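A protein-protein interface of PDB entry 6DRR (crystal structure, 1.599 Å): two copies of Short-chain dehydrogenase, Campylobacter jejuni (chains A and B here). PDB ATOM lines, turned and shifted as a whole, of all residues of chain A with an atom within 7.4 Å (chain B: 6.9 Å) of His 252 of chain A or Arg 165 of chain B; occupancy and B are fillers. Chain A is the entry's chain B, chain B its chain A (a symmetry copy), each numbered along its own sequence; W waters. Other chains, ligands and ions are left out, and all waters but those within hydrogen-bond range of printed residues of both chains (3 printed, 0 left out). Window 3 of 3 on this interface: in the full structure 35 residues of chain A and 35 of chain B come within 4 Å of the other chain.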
ATOM      1  N   ILE A 144       9.464  -1.758 -21.274  1.00  0.00           N
ATOM      2  CA  ILE A 144       9.043  -0.429 -20.827  1.00  0.00           C
ATOM      3  C   ILE A 144       8.930   0.542 -21.994  1.00  0.00           C
ATOM      4  O   ILE A 144       7.953   1.285 -22.107  1.00  0.00           O
ATOM      5  CB  ILE A 144      10.050   0.098 -19.778  1.00  0.00           C
ATOM      6  CG1 ILE A 144      10.154  -0.859 -18.592  1.00  0.00           C
ATOM      7  CG2 ILE A 144       9.672   1.505 -19.319  1.00  0.00           C
ATOM      8  CD1 ILE A 144      11.392  -0.635 -17.737  1.00  0.00           C
ATOM      9  N   THR A 145       9.949   0.566 -22.853  1.00  0.00           N
ATOM     10  CA  THR A 145      10.085   1.576 -23.896  1.00  0.00           C
ATOM     11  C   THR A 145       9.545   1.126 -25.244  1.00  0.00           C
ATOM     12  O   THR A 145       9.319   1.977 -26.116  1.00  0.00           O
ATOM     13  CB  THR A 145      11.567   1.958 -24.093  1.00  0.00           C
ATOM     14  OG1 THR A 145      12.269   0.856 -24.673  1.00  0.00           O
ATOM     15  CG2 THR A 145      12.226   2.323 -22.771  1.00  0.00           C
ATOM     16  N   PRO A 213      23.567   7.764 -22.348  1.00  0.00           N
ATOM     17  CA  PRO A 213      24.140   8.990 -21.772  1.00  0.00           C
ATOM     18  C   PRO A 213      25.422   8.777 -20.982  1.00  0.00           C
ATOM     19  O   PRO A 213      26.364   9.574 -21.108  1.00  0.00           O
ATOM     20  CB  PRO A 213      22.996   9.498 -20.879  1.00  0.00           C
ATOM     21  CG  PRO A 213      21.762   8.984 -21.546  1.00  0.00           C
ATOM     22  CD  PRO A 213      22.120   7.648 -22.107  1.00  0.00           C
ATOM     23  N   ILE A 243      11.469  -2.496 -10.216  1.00  0.00           N
ATOM     24  CA  ILE A 243      12.052  -2.693 -11.537  1.00  0.00           C
ATOM     25  C   ILE A 243      13.256  -1.766 -11.605  1.00  0.00           C
ATOM     26  O   ILE A 243      13.105  -0.539 -11.652  1.00  0.00           O
ATOM     27  CB  ILE A 243      11.050  -2.411 -12.664  1.00  0.00           C
ATOM     28  CG1 ILE A 243       9.813  -3.306 -12.506  1.00  0.00           C
ATOM     29  CG2 ILE A 243      11.706  -2.645 -14.024  1.00  0.00           C
ATOM     30  CD1 ILE A 243       8.586  -2.785 -13.204  1.00  0.00           C
ATOM     31  N   LEU A 244      14.448  -2.355 -11.567  1.00  0.00           N
ATOM     32  CA  LEU A 244      15.698  -1.633 -11.406  1.00  0.00           C
ATOM     33  C   LEU A 244      16.368  -1.438 -12.753  1.00  0.00           C
ATOM     34  O   LEU A 244      16.428  -2.364 -13.563  1.00  0.00           O
ATOM     35  CB  LEU A 244      16.636  -2.387 -10.464  1.00  0.00           C
ATOM     36  CG  LEU A 244      16.064  -2.695  -9.082  1.00  0.00           C
ATOM     37  CD1 LEU A 244      17.060  -3.565  -8.286  1.00  0.00           C
ATOM     38  CD2 LEU A 244      15.744  -1.400  -8.335  1.00  0.00           C
ATOM     39  N   MET A 245      16.874  -0.229 -12.988  1.00  0.00           N
ATOM     40  CA  MET A 245      17.497   0.150 -14.254  1.00  0.00           C
ATOM     41  C   MET A 245      18.931   0.603 -14.025  1.00  0.00           C
ATOM     42  O   MET A 245      19.186   1.802 -13.845  1.00  0.00           O
ATOM     43  CB  MET A 245      16.712   1.259 -14.961  1.00  0.00           C
ATOM     44  CG  MET A 245      15.436   0.864 -15.654  1.00  0.00           C
ATOM     45  SD  MET A 245      14.189   0.561 -14.434  1.00  0.00           S
ATOM     46  CE  MET A 245      12.825   1.572 -14.994  1.00  0.00           C
ATOM     47  N   ASP A 247      21.430   1.252 -16.317  1.00  0.00           N
ATOM     48  CA  ASP A 247      21.289   1.244 -17.768  1.00  0.00           C
ATOM     49  C   ASP A 247      21.943   2.449 -18.435  1.00  0.00           C
ATOM     50  O   ASP A 247      21.689   2.704 -19.622  1.00  0.00           O
ATOM     51  CB  ASP A 247      19.797   1.134 -18.170  1.00  0.00           C
ATOM     52  CG  ASP A 247      18.980   2.409 -17.897  1.00  0.00           C
ATOM     53  OD1 ASP A 247      19.472   3.358 -17.248  1.00  0.00           O
ATOM     54  OD2 ASP A 247      17.811   2.455 -18.342  1.00  0.00           O
ATOM     55  N   GLY A 248      22.786   3.187 -17.714  1.00  0.00           N
ATOM     56  CA  GLY A 248      23.454   4.331 -18.297  1.00  0.00           C
ATOM     57  C   GLY A 248      22.562   5.526 -18.531  1.00  0.00           C
ATOM     58  O   GLY A 248      23.005   6.487 -19.157  1.00  0.00           O
ATOM     59  N   GLY A 249      21.328   5.501 -18.027  1.00  0.00           N
ATOM     60  CA  GLY A 249      20.375   6.560 -18.268  1.00  0.00           C
ATOM     61  C   GLY A 249      19.444   6.323 -19.433  1.00  0.00           C
ATOM     62  O   GLY A 249      18.728   7.248 -19.823  1.00  0.00           O
ATOM     63  N   TYR A 250      19.409   5.102 -19.978  1.00  0.00           N
ATOM     64  CA  TYR A 250      18.705   4.850 -21.234  1.00  0.00           C
ATOM     65  C   TYR A 250      17.203   5.123 -21.120  1.00  0.00           C
ATOM     66  O   TYR A 250      16.602   5.746 -22.005  1.00  0.00           O
ATOM     67  CB  TYR A 250      18.960   3.402 -21.674  1.00  0.00           C
ATOM     68  CG  TYR A 250      18.560   3.094 -23.092  1.00  0.00           C
ATOM     69  CD1 TYR A 250      17.216   2.989 -23.455  1.00  0.00           C
ATOM     70  CD2 TYR A 250      19.525   2.887 -24.069  1.00  0.00           C
ATOM     71  CE1 TYR A 250      16.850   2.725 -24.758  1.00  0.00           C
ATOM     72  CE2 TYR A 250      19.176   2.620 -25.373  1.00  0.00           C
ATOM     73  CZ  TYR A 250      17.845   2.529 -25.711  1.00  0.00           C
ATOM     74  OH  TYR A 250      17.518   2.260 -27.011  1.00  0.00           O
ATOM     75  N   VAL A 251      16.571   4.625 -20.062  1.00  0.00           N
ATOM     76  CA  VAL A 251      15.124   4.768 -19.952  1.00  0.00           C
ATOM     77  C   VAL A 251      14.733   6.177 -19.526  1.00  0.00           C
ATOM     78  O   VAL A 251      13.724   6.709 -20.004  1.00  0.00           O
ATOM     79  CB  VAL A 251      14.566   3.706 -18.986  1.00  0.00           C
ATOM     80  CG1 VAL A 251      13.118   4.011 -18.628  1.00  0.00           C
ATOM     81  CG2 VAL A 251      14.668   2.333 -19.628  1.00  0.00           C
ATOM     82  N   HIS A 252      15.493   6.809 -18.615  1.00  0.00           N
ATOM     83  CA  HIS A 252      14.914   7.941 -17.897  1.00  0.00           C
ATOM     84  C   HIS A 252      15.407   9.311 -18.335  1.00  0.00           C
ATOM     85  O   HIS A 252      14.731  10.305 -18.044  1.00  0.00           O
ATOM     86  CB  HIS A 252      15.162   7.797 -16.390  1.00  0.00           C
ATOM     87  CG  HIS A 252      14.474   6.613 -15.793  1.00  0.00           C
ATOM     88  ND1 HIS A 252      15.143   5.463 -15.441  1.00  0.00           N
ATOM     89  CD2 HIS A 252      13.167   6.388 -15.522  1.00  0.00           C
ATOM     90  CE1 HIS A 252      14.283   4.583 -14.964  1.00  0.00           C
ATOM     91  NE2 HIS A 252      13.076   5.123 -14.994  1.00  0.00           N
ATOM     92  N   LEU A 253      16.556   9.407 -18.988  1.00  0.00           N
ATOM     93  CA  LEU A 253      17.102  10.720 -19.302  1.00  0.00           C
ATOM     94  C   LEU A 253      16.658  11.191 -20.679  1.00  0.00           C
ATOM     95  O   LEU A 253      16.427  10.392 -21.587  1.00  0.00           O
ATOM     96  CB  LEU A 253      18.628  10.705 -19.228  1.00  0.00           C
ATOM     97  CG  LEU A 253      19.181  10.251 -17.871  1.00  0.00           C
ATOM     98  CD1 LEU A 253      20.682  10.499 -17.829  1.00  0.00           C
ATOM     99  CD2 LEU A 253      18.462  10.960 -16.699  1.00  0.00           C
ATOM    100  N   ASP A 254      16.543  12.509 -20.819  1.00  0.00           N
ATOM    101  CA  ASP A 254      16.124  13.171 -22.055  1.00  0.00           C
ATOM    102  C   ASP A 254      16.654  12.474 -23.310  1.00  0.00           C
ATOM    103  O   ASP A 254      17.864  12.326 -23.490  1.00  0.00           O
ATOM    104  CB  ASP A 254      16.609  14.625 -22.016  1.00  0.00           C
ATOM    105  CG  ASP A 254      16.074  15.464 -23.158  1.00  0.00           C
ATOM    106  OD1 ASP A 254      15.321  14.957 -24.029  1.00  0.00           O
ATOM    107  OD2 ASP A 254      16.426  16.661 -23.189  1.00  0.00           O
ATOM    108  N   ARG A 255      15.734  12.054 -24.191  1.00  0.00           N
ATOM    109  CA  ARG A 255      16.120  11.368 -25.424  1.00  0.00           C
ATOM    110  C   ARG A 255      17.026  12.218 -26.302  1.00  0.00           C
ATOM    111  O   ARG A 255      17.773  11.666 -27.118  1.00  0.00           O
ATOM    112  CB  ARG A 255      14.875  10.961 -26.225  1.00  0.00           C
ATOM    113  CG  ARG A 255      14.105  12.151 -26.812  1.00  0.00           C
ATOM    114  CD  ARG A 255      12.661  11.801 -27.184  1.00  0.00           C
ATOM    115  NE  ARG A 255      12.603  10.707 -28.149  1.00  0.00           N
ATOM    116  CZ  ARG A 255      12.249   9.455 -27.842  1.00  0.00           C
ATOM    117  NH1 ARG A 255      11.924   9.127 -26.596  1.00  0.00           N
ATOM    118  NH2 ARG A 255      12.257   8.522 -28.779  1.00  0.00           N
ATOM    119  N   LEU A 257      19.518  14.081 -25.340  1.00  0.00           N
ATOM    120  CA  LEU A 257      20.816  14.346 -24.734  1.00  0.00           C
ATOM    121  C   LEU A 257      21.936  13.958 -25.693  1.00  0.00           C
ATOM    122  O   LEU A 257      21.906  12.886 -26.307  1.00  0.00           O
ATOM    123  CB  LEU A 257      20.940  13.574 -23.418  1.00  0.00           C
ATOM    124  CG  LEU A 257      22.087  13.928 -22.481  1.00  0.00           C
ATOM    125  CD1 LEU A 257      21.996  15.371 -22.057  1.00  0.00           C
ATOM    126  CD2 LEU A 257      22.030  13.004 -21.269  1.00  0.00           C
ATOM    127  N   ASN B 137      20.877  12.082  -3.726  1.00  0.00           N
ATOM    128  CA  ASN B 137      19.879  12.938  -3.096  1.00  0.00           C
ATOM    129  C   ASN B 137      18.913  12.075  -2.294  1.00  0.00           C
ATOM    130  O   ASN B 137      18.209  11.234  -2.863  1.00  0.00           O
ATOM    131  CB  ASN B 137      19.129  13.748  -4.157  1.00  0.00           C
ATOM    132  CG  ASN B 137      20.021  14.736  -4.862  1.00  0.00           C
ATOM    133  OD1 ASN B 137      20.851  15.406  -4.230  1.00  0.00           O
ATOM    134  ND2 ASN B 137      19.878  14.832  -6.183  1.00  0.00           N
ATOM    135  N   GLN B 160      13.728  17.840  -5.805  1.00  0.00           N
ATOM    136  CA  GLN B 160      15.024  17.174  -5.731  1.00  0.00           C
ATOM    137  C   GLN B 160      15.081  15.949  -6.629  1.00  0.00           C
ATOM    138  O   GLN B 160      16.171  15.574  -7.077  1.00  0.00           O
ATOM    139  CB  GLN B 160      15.331  16.797  -4.284  1.00  0.00           C
ATOM    140  CG  GLN B 160      15.507  18.046  -3.409  1.00  0.00           C
ATOM    141  CD  GLN B 160      15.342  17.765  -1.933  1.00  0.00           C
ATOM    142  OE1 GLN B 160      14.969  16.666  -1.539  1.00  0.00           O
ATOM    143  NE2 GLN B 160      15.640  18.764  -1.103  1.00  0.00           N
ATOM    144  N   MET B 161      13.931  15.308  -6.884  1.00  0.00           N
ATOM    145  CA  MET B 161      13.875  14.307  -7.950  1.00  0.00           C
ATOM    146  C   MET B 161      14.164  14.940  -9.301  1.00  0.00           C
ATOM    147  O   MET B 161      14.869  14.353 -10.127  1.00  0.00           O
ATOM    148  CB  MET B 161      12.518  13.609  -7.949  1.00  0.00           C
ATOM    149  CG  MET B 161      12.290  12.875  -6.643  1.00  0.00           C
ATOM    150  SD  MET B 161      10.841  11.810  -6.674  1.00  0.00           S
ATOM    151  CE  MET B 161       9.533  12.994  -6.759  1.00  0.00           C
ATOM    152  N   GLY B 162      13.645  16.147  -9.530  1.00  0.00           N
ATOM    153  CA  GLY B 162      13.978  16.873 -10.747  1.00  0.00           C
ATOM    154  C   GLY B 162      15.453  17.216 -10.864  1.00  0.00           C
ATOM    155  O   GLY B 162      16.054  17.060 -11.929  1.00  0.00           O
ATOM    156  N   PHE B 163      16.053  17.702  -9.777  1.00  0.00           N
ATOM    157  CA  PHE B 163      17.499  17.896  -9.774  1.00  0.00           C
ATOM    158  C   PHE B 163      18.227  16.600 -10.113  1.00  0.00           C
ATOM    159  O   PHE B 163      19.241  16.611 -10.823  1.00  0.00           O
ATOM    160  CB  PHE B 163      17.975  18.383  -8.404  1.00  0.00           C
ATOM    161  CG  PHE B 163      17.794  19.868  -8.144  1.00  0.00           C
ATOM    162  CD1 PHE B 163      18.068  20.835  -9.114  1.00  0.00           C
ATOM    163  CD2 PHE B 163      17.373  20.287  -6.886  1.00  0.00           C
ATOM    164  CE1 PHE B 163      17.925  22.205  -8.818  1.00  0.00           C
ATOM    165  CE2 PHE B 163      17.206  21.638  -6.590  1.00  0.00           C
ATOM    166  CZ  PHE B 163      17.482  22.599  -7.559  1.00  0.00           C
ATOM    167  N   THR B 164      17.747  15.476  -9.584  1.00  0.00           N
ATOM    168  CA  THR B 164      18.426  14.206  -9.817  1.00  0.00           C
ATOM    169  C   THR B 164      18.471  13.886 -11.304  1.00  0.00           C
ATOM    170  O   THR B 164      19.527  13.544 -11.844  1.00  0.00           O
ATOM    171  CB  THR B 164      17.727  13.075  -9.059  1.00  0.00           C
ATOM    172  OG1 THR B 164      17.778  13.346  -7.656  1.00  0.00           O
ATOM    173  CG2 THR B 164      18.423  11.736  -9.337  1.00  0.00           C
ATOM    174  N   ARG B 165      17.328  14.011 -11.979  1.00  0.00           N
ATOM    175  CA  ARG B 165      17.283  13.772 -13.421  1.00  0.00           C
ATOM    176  C   ARG B 165      18.077  14.824 -14.188  1.00  0.00           C
ATOM    177  O   ARG B 165      18.814  14.494 -15.129  1.00  0.00           O
ATOM    178  CB  ARG B 165      15.825  13.744 -13.899  1.00  0.00           C
ATOM    179  CG  ARG B 165      15.038  12.526 -13.369  1.00  0.00           C
ATOM    180  CD  ARG B 165      15.340  11.274 -14.205  1.00  0.00           C
ATOM    181  NE  ARG B 165      14.903  10.041 -13.537  1.00  0.00           N
ATOM    182  CZ  ARG B 165      13.645   9.611 -13.496  1.00  0.00           C
ATOM    183  NH1 ARG B 165      12.668  10.297 -14.095  1.00  0.00           N
ATOM    184  NH2 ARG B 165      13.355   8.482 -12.848  1.00  0.00           N
ATOM    185  N   GLU B 166      17.952  16.090 -13.792  1.00  0.00           N
ATOM    186  CA  GLU B 166      18.643  17.164 -14.504  1.00  0.00           C
ATOM    187  C   GLU B 166      20.160  17.035 -14.385  1.00  0.00           C
ATOM    188  O   GLU B 166      20.884  17.138 -15.384  1.00  0.00           O
ATOM    189  CB  GLU B 166      18.164  18.505 -13.965  1.00  0.00           C
ATOM    190  CG  GLU B 166      19.061  19.667 -14.309  1.00  0.00           C
ATOM    191  CD  GLU B 166      19.042  20.023 -15.774  1.00  0.00           C
ATOM    192  OE1 GLU B 166      18.165  19.543 -16.528  1.00  0.00           O
ATOM    193  OE2 GLU B 166      19.924  20.814 -16.164  1.00  0.00           O
ATOM    194  N   TRP B 167      20.660  16.805 -13.169  1.00  0.00           N
ATOM    195  CA  TRP B 167      22.105  16.682 -12.974  1.00  0.00           C
ATOM    196  C   TRP B 167      22.629  15.395 -13.581  1.00  0.00           C
ATOM    197  O   TRP B 167      23.772  15.357 -14.054  1.00  0.00           O
ATOM    198  CB  TRP B 167      22.460  16.751 -11.486  1.00  0.00           C
ATOM    199  CG  TRP B 167      22.074  18.063 -10.833  1.00  0.00           C
ATOM    200  CD1 TRP B 167      21.876  19.274 -11.458  1.00  0.00           C
ATOM    201  CD2 TRP B 167      21.833  18.288  -9.438  1.00  0.00           C
ATOM    202  NE1 TRP B 167      21.514  20.223 -10.532  1.00  0.00           N
ATOM    203  CE2 TRP B 167      21.486  19.649  -9.287  1.00  0.00           C
ATOM    204  CE3 TRP B 167      21.862  17.467  -8.301  1.00  0.00           C
ATOM    205  CZ2 TRP B 167      21.179  20.209  -8.040  1.00  0.00           C
ATOM    206  CZ3 TRP B 167      21.562  18.023  -7.063  1.00  0.00           C
ATOM    207  CH2 TRP B 167      21.230  19.384  -6.944  1.00  0.00           C
ATOM    208  N   ALA B 168      21.814  14.338 -13.604  1.00  0.00           N
ATOM    209  CA  ALA B 168      22.234  13.134 -14.314  1.00  0.00           C
ATOM    210  C   ALA B 168      22.475  13.426 -15.791  1.00  0.00           C
ATOM    211  O   ALA B 168      23.489  12.994 -16.353  1.00  0.00           O
ATOM    212  CB  ALA B 168      21.197  12.020 -14.137  1.00  0.00           C
ATOM    213  N   CYS B 169      21.566  14.178 -16.426  1.00  0.00           N
ATOM    214  CA  CYS B 169      21.786  14.644 -17.794  1.00  0.00           C
ATOM    215  C   CYS B 169      23.034  15.513 -17.895  1.00  0.00           C
ATOM    216  O   CYS B 169      23.833  15.364 -18.827  1.00  0.00           O
ATOM    217  CB  CYS B 169      20.586  15.453 -18.279  1.00  0.00           C
ATOM    218  SG  CYS B 169      19.094  14.505 -18.655  1.00  0.00           S
ATOM    219  N   ALA B 170      23.174  16.478 -16.976  1.00  0.00           N
ATOM    220  CA  ALA B 170      24.230  17.485 -17.093  1.00  0.00           C
ATOM    221  C   ALA B 170      25.613  16.864 -17.046  1.00  0.00           C
ATOM    222  O   ALA B 170      26.528  17.318 -17.743  1.00  0.00           O
ATOM    223  CB  ALA B 170      24.088  18.518 -15.971  1.00  0.00           C
ATOM    224  N   VAL B 178      24.322  10.523 -10.746  1.00  0.00           N
ATOM    225  CA  VAL B 178      23.432  11.262  -9.845  1.00  0.00           C
ATOM    226  C   VAL B 178      22.170  10.441  -9.638  1.00  0.00           C
ATOM    227  O   VAL B 178      21.431  10.187 -10.594  1.00  0.00           O
ATOM    228  CB  VAL B 178      23.075  12.652 -10.398  1.00  0.00           C
ATOM    229  CG1 VAL B 178      22.256  13.438  -9.379  1.00  0.00           C
ATOM    230  CG2 VAL B 178      24.356  13.418 -10.776  1.00  0.00           C
ATOM    231  N   THR B 240      22.497   5.769 -13.181  1.00  0.00           N
ATOM    232  CA  THR B 240      22.342   7.205 -13.015  1.00  0.00           C
ATOM    233  C   THR B 240      20.918   7.620 -13.353  1.00  0.00           C
ATOM    234  O   THR B 240      20.205   6.953 -14.111  1.00  0.00           O
ATOM    235  CB  THR B 240      23.366   7.974 -13.858  1.00  0.00           C
ATOM    236  OG1 THR B 240      23.421   9.335 -13.421  1.00  0.00           O
ATOM    237  CG2 THR B 240      22.976   7.942 -15.322  1.00  0.00           C
ATOM    238  N   GLY B 241      20.516   8.752 -12.778  1.00  0.00           N
ATOM    239  CA  GLY B 241      19.163   9.240 -12.940  1.00  0.00           C
ATOM    240  C   GLY B 241      18.101   8.439 -12.220  1.00  0.00           C
ATOM    241  O   GLY B 241      16.911   8.638 -12.486  1.00  0.00           O
ATOM    242  N   GLN B 242      18.482   7.545 -11.317  1.00  0.00           N
ATOM    243  CA  GLN B 242      17.520   6.629 -10.711  1.00  0.00           C
ATOM    244  C   GLN B 242      16.917   7.207  -9.438  1.00  0.00           C
ATOM    245  O   GLN B 242      17.611   7.831  -8.634  1.00  0.00           O
ATOM    246  CB  GLN B 242      18.185   5.290 -10.396  1.00  0.00           C
ATOM    247  CG  GLN B 242      18.655   4.592 -11.642  1.00  0.00           C
ATOM    248  CD  GLN B 242      17.551   4.556 -12.672  1.00  0.00           C
ATOM    249  OE1 GLN B 242      16.533   3.908 -12.459  1.00  0.00           O
ATOM    250  NE2 GLN B 242      17.729   5.284 -13.774  1.00  0.00           N
ATOM    251  N   ILE B 243      15.613   7.003  -9.282  1.00  0.00           N
ATOM    252  CA  ILE B 243      14.916   7.233  -8.025  1.00  0.00           C
ATOM    253  C   ILE B 243      14.659   5.855  -7.439  1.00  0.00           C
ATOM    254  O   ILE B 243      13.825   5.105  -7.953  1.00  0.00           O
ATOM    255  CB  ILE B 243      13.604   8.002  -8.217  1.00  0.00           C
ATOM    256  CG1 ILE B 243      13.794   9.241  -9.093  1.00  0.00           C
ATOM    257  CG2 ILE B 243      13.009   8.357  -6.845  1.00  0.00           C
ATOM    258  CD1 ILE B 243      14.769  10.203  -8.566  1.00  0.00           C
HETATM  259  O   HOH W   1      17.482   5.390 -17.066  1.00  0.00           O
HETATM  260  O   HOH W   2      20.662   3.831 -14.662  1.00  0.00           O
HETATM  261  O   HOH W   3      16.727   1.718 -10.831  1.00  0.00           O
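Water W2 lies within hydrogen-bond range of the backbone carbonyl oxygen (O) of Met 245 of chain A, the side-chain carboxylate (OD1) of Asp 247 of chain A, the backbone NH (N) of Thr 240 of chain B and the side-chain amide nitrogen (NE2) of Gln 242 of chain B. Water W3 bridges the side-chain amide oxygen (OE1) of Gln 242 of chain B (2.7 Å) and the backbone NH (N) of Met 245 of chain A (2.9 Å). Water W1 lies within hydrogen-bond range of ND1 of His 252 of chain A, OD1 of Asp 247 of chain A, N of Val 251 of chain A and NE2 of Gln 242 of chain B.
O of Met 245 of chain A touches CD of Gln 242 of chain B (3.4 Å). Gly 249 of chain A touches Thr 240 of chain B (N to CG2, 3.999 Å). CD2 of His 252 of chain A touches NH2 of Arg 165 of chain B, 3.4 Å away. Leu 253 of chain A touches Arg 165 of chain B. Leu 253 of chain A touches Ala 168 of chain B. Leu 253 of chain A touches Cys 169 of chain B. Asp 254 of chain A touches Cys 169 of chain B. Cys 169 of chain B touches Leu 257 of chain A (O to CD1, 3.7 Å).
The side-chain carboxylate of Asp 247 of chain A lies within hydrogen-bond range of the backbone NH of Gly 249 of chain A (2.9 Å). The backbone carbonyl oxygen (O) of Thr 240 of chain B sits at hydrogen-bond distance from the side-chain amide nitrogen (NE2) of Gln 242 of chain B, 3.0 Å away. The guanidinium group (NE) of Arg 165 of chain B lies within hydrogen-bond range of the backbone carbonyl oxygen (O) of Gly 241 of chain B. The side-chain sulfur of Cys 169 of chain B sits at hydrogen-bond distance from the backbone carbonyl oxygen of Arg 165 of chain B (3.5 Å). OG1 of Thr 240 of chain B is in hydrogen-bond range of N of Val 178 of chain B, at 3.1 Å.
1 position is printed for both chains. Of the 9 pairs that touch across the chains among the printed residues, none has its exchanged pair printed and touching as well.
His 252 of chain A touches just these residues of chain B: Arg 165 (3.4 Å) and Gln 242 (3.1 Å). Of chain A, only His 252 and Leu 253 come within 4 Å of Arg 165 of chain B. Printed residues of chain B within 4 Å of Gly 249 of chain A: Thr 240 (3.999 Å). Of the printed residues of chain B, Asp 254 of chain A touches Cys 169. Printed residues of chain A within 4 Å of Ala 168 of chain B: Leu 253 (3.9 Å). Of the printed residues of chain B, Leu 257 of chain A touches Cys 169. Gln 160 of chain B touches none of the printed residues of chain A. The nearest residue of chain B that does not touch His 252 of chain A is Gly 241 of chain B (4.4 Å). The nearest printed residue of chain A that does not touch Cys 169 of chain B is His 252 of chain A (6.1 Å).
Hydrophobic or aromatic side chains of chain A within 4 Å of the printed part of chain B: Met 245, His 252, Leu 253 and Leu 257. Of the 17 printed residues of chain B, 5 touch a printed residue of chain A. Printed residues of chain B that touch a printed residue of chain A: Arg 165, Ala 168, Cys 169, Thr 240 and Gln 242. Hydrophobic or aromatic side chains of chain B that line the printed part of chain A: Ala 168.
The side-chain amide nitrogen of Gln 242 of chain B lies within hydrogen-bond range of a ring nitrogen (ND1) of His 252 of chain A, 3.1 Å away.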
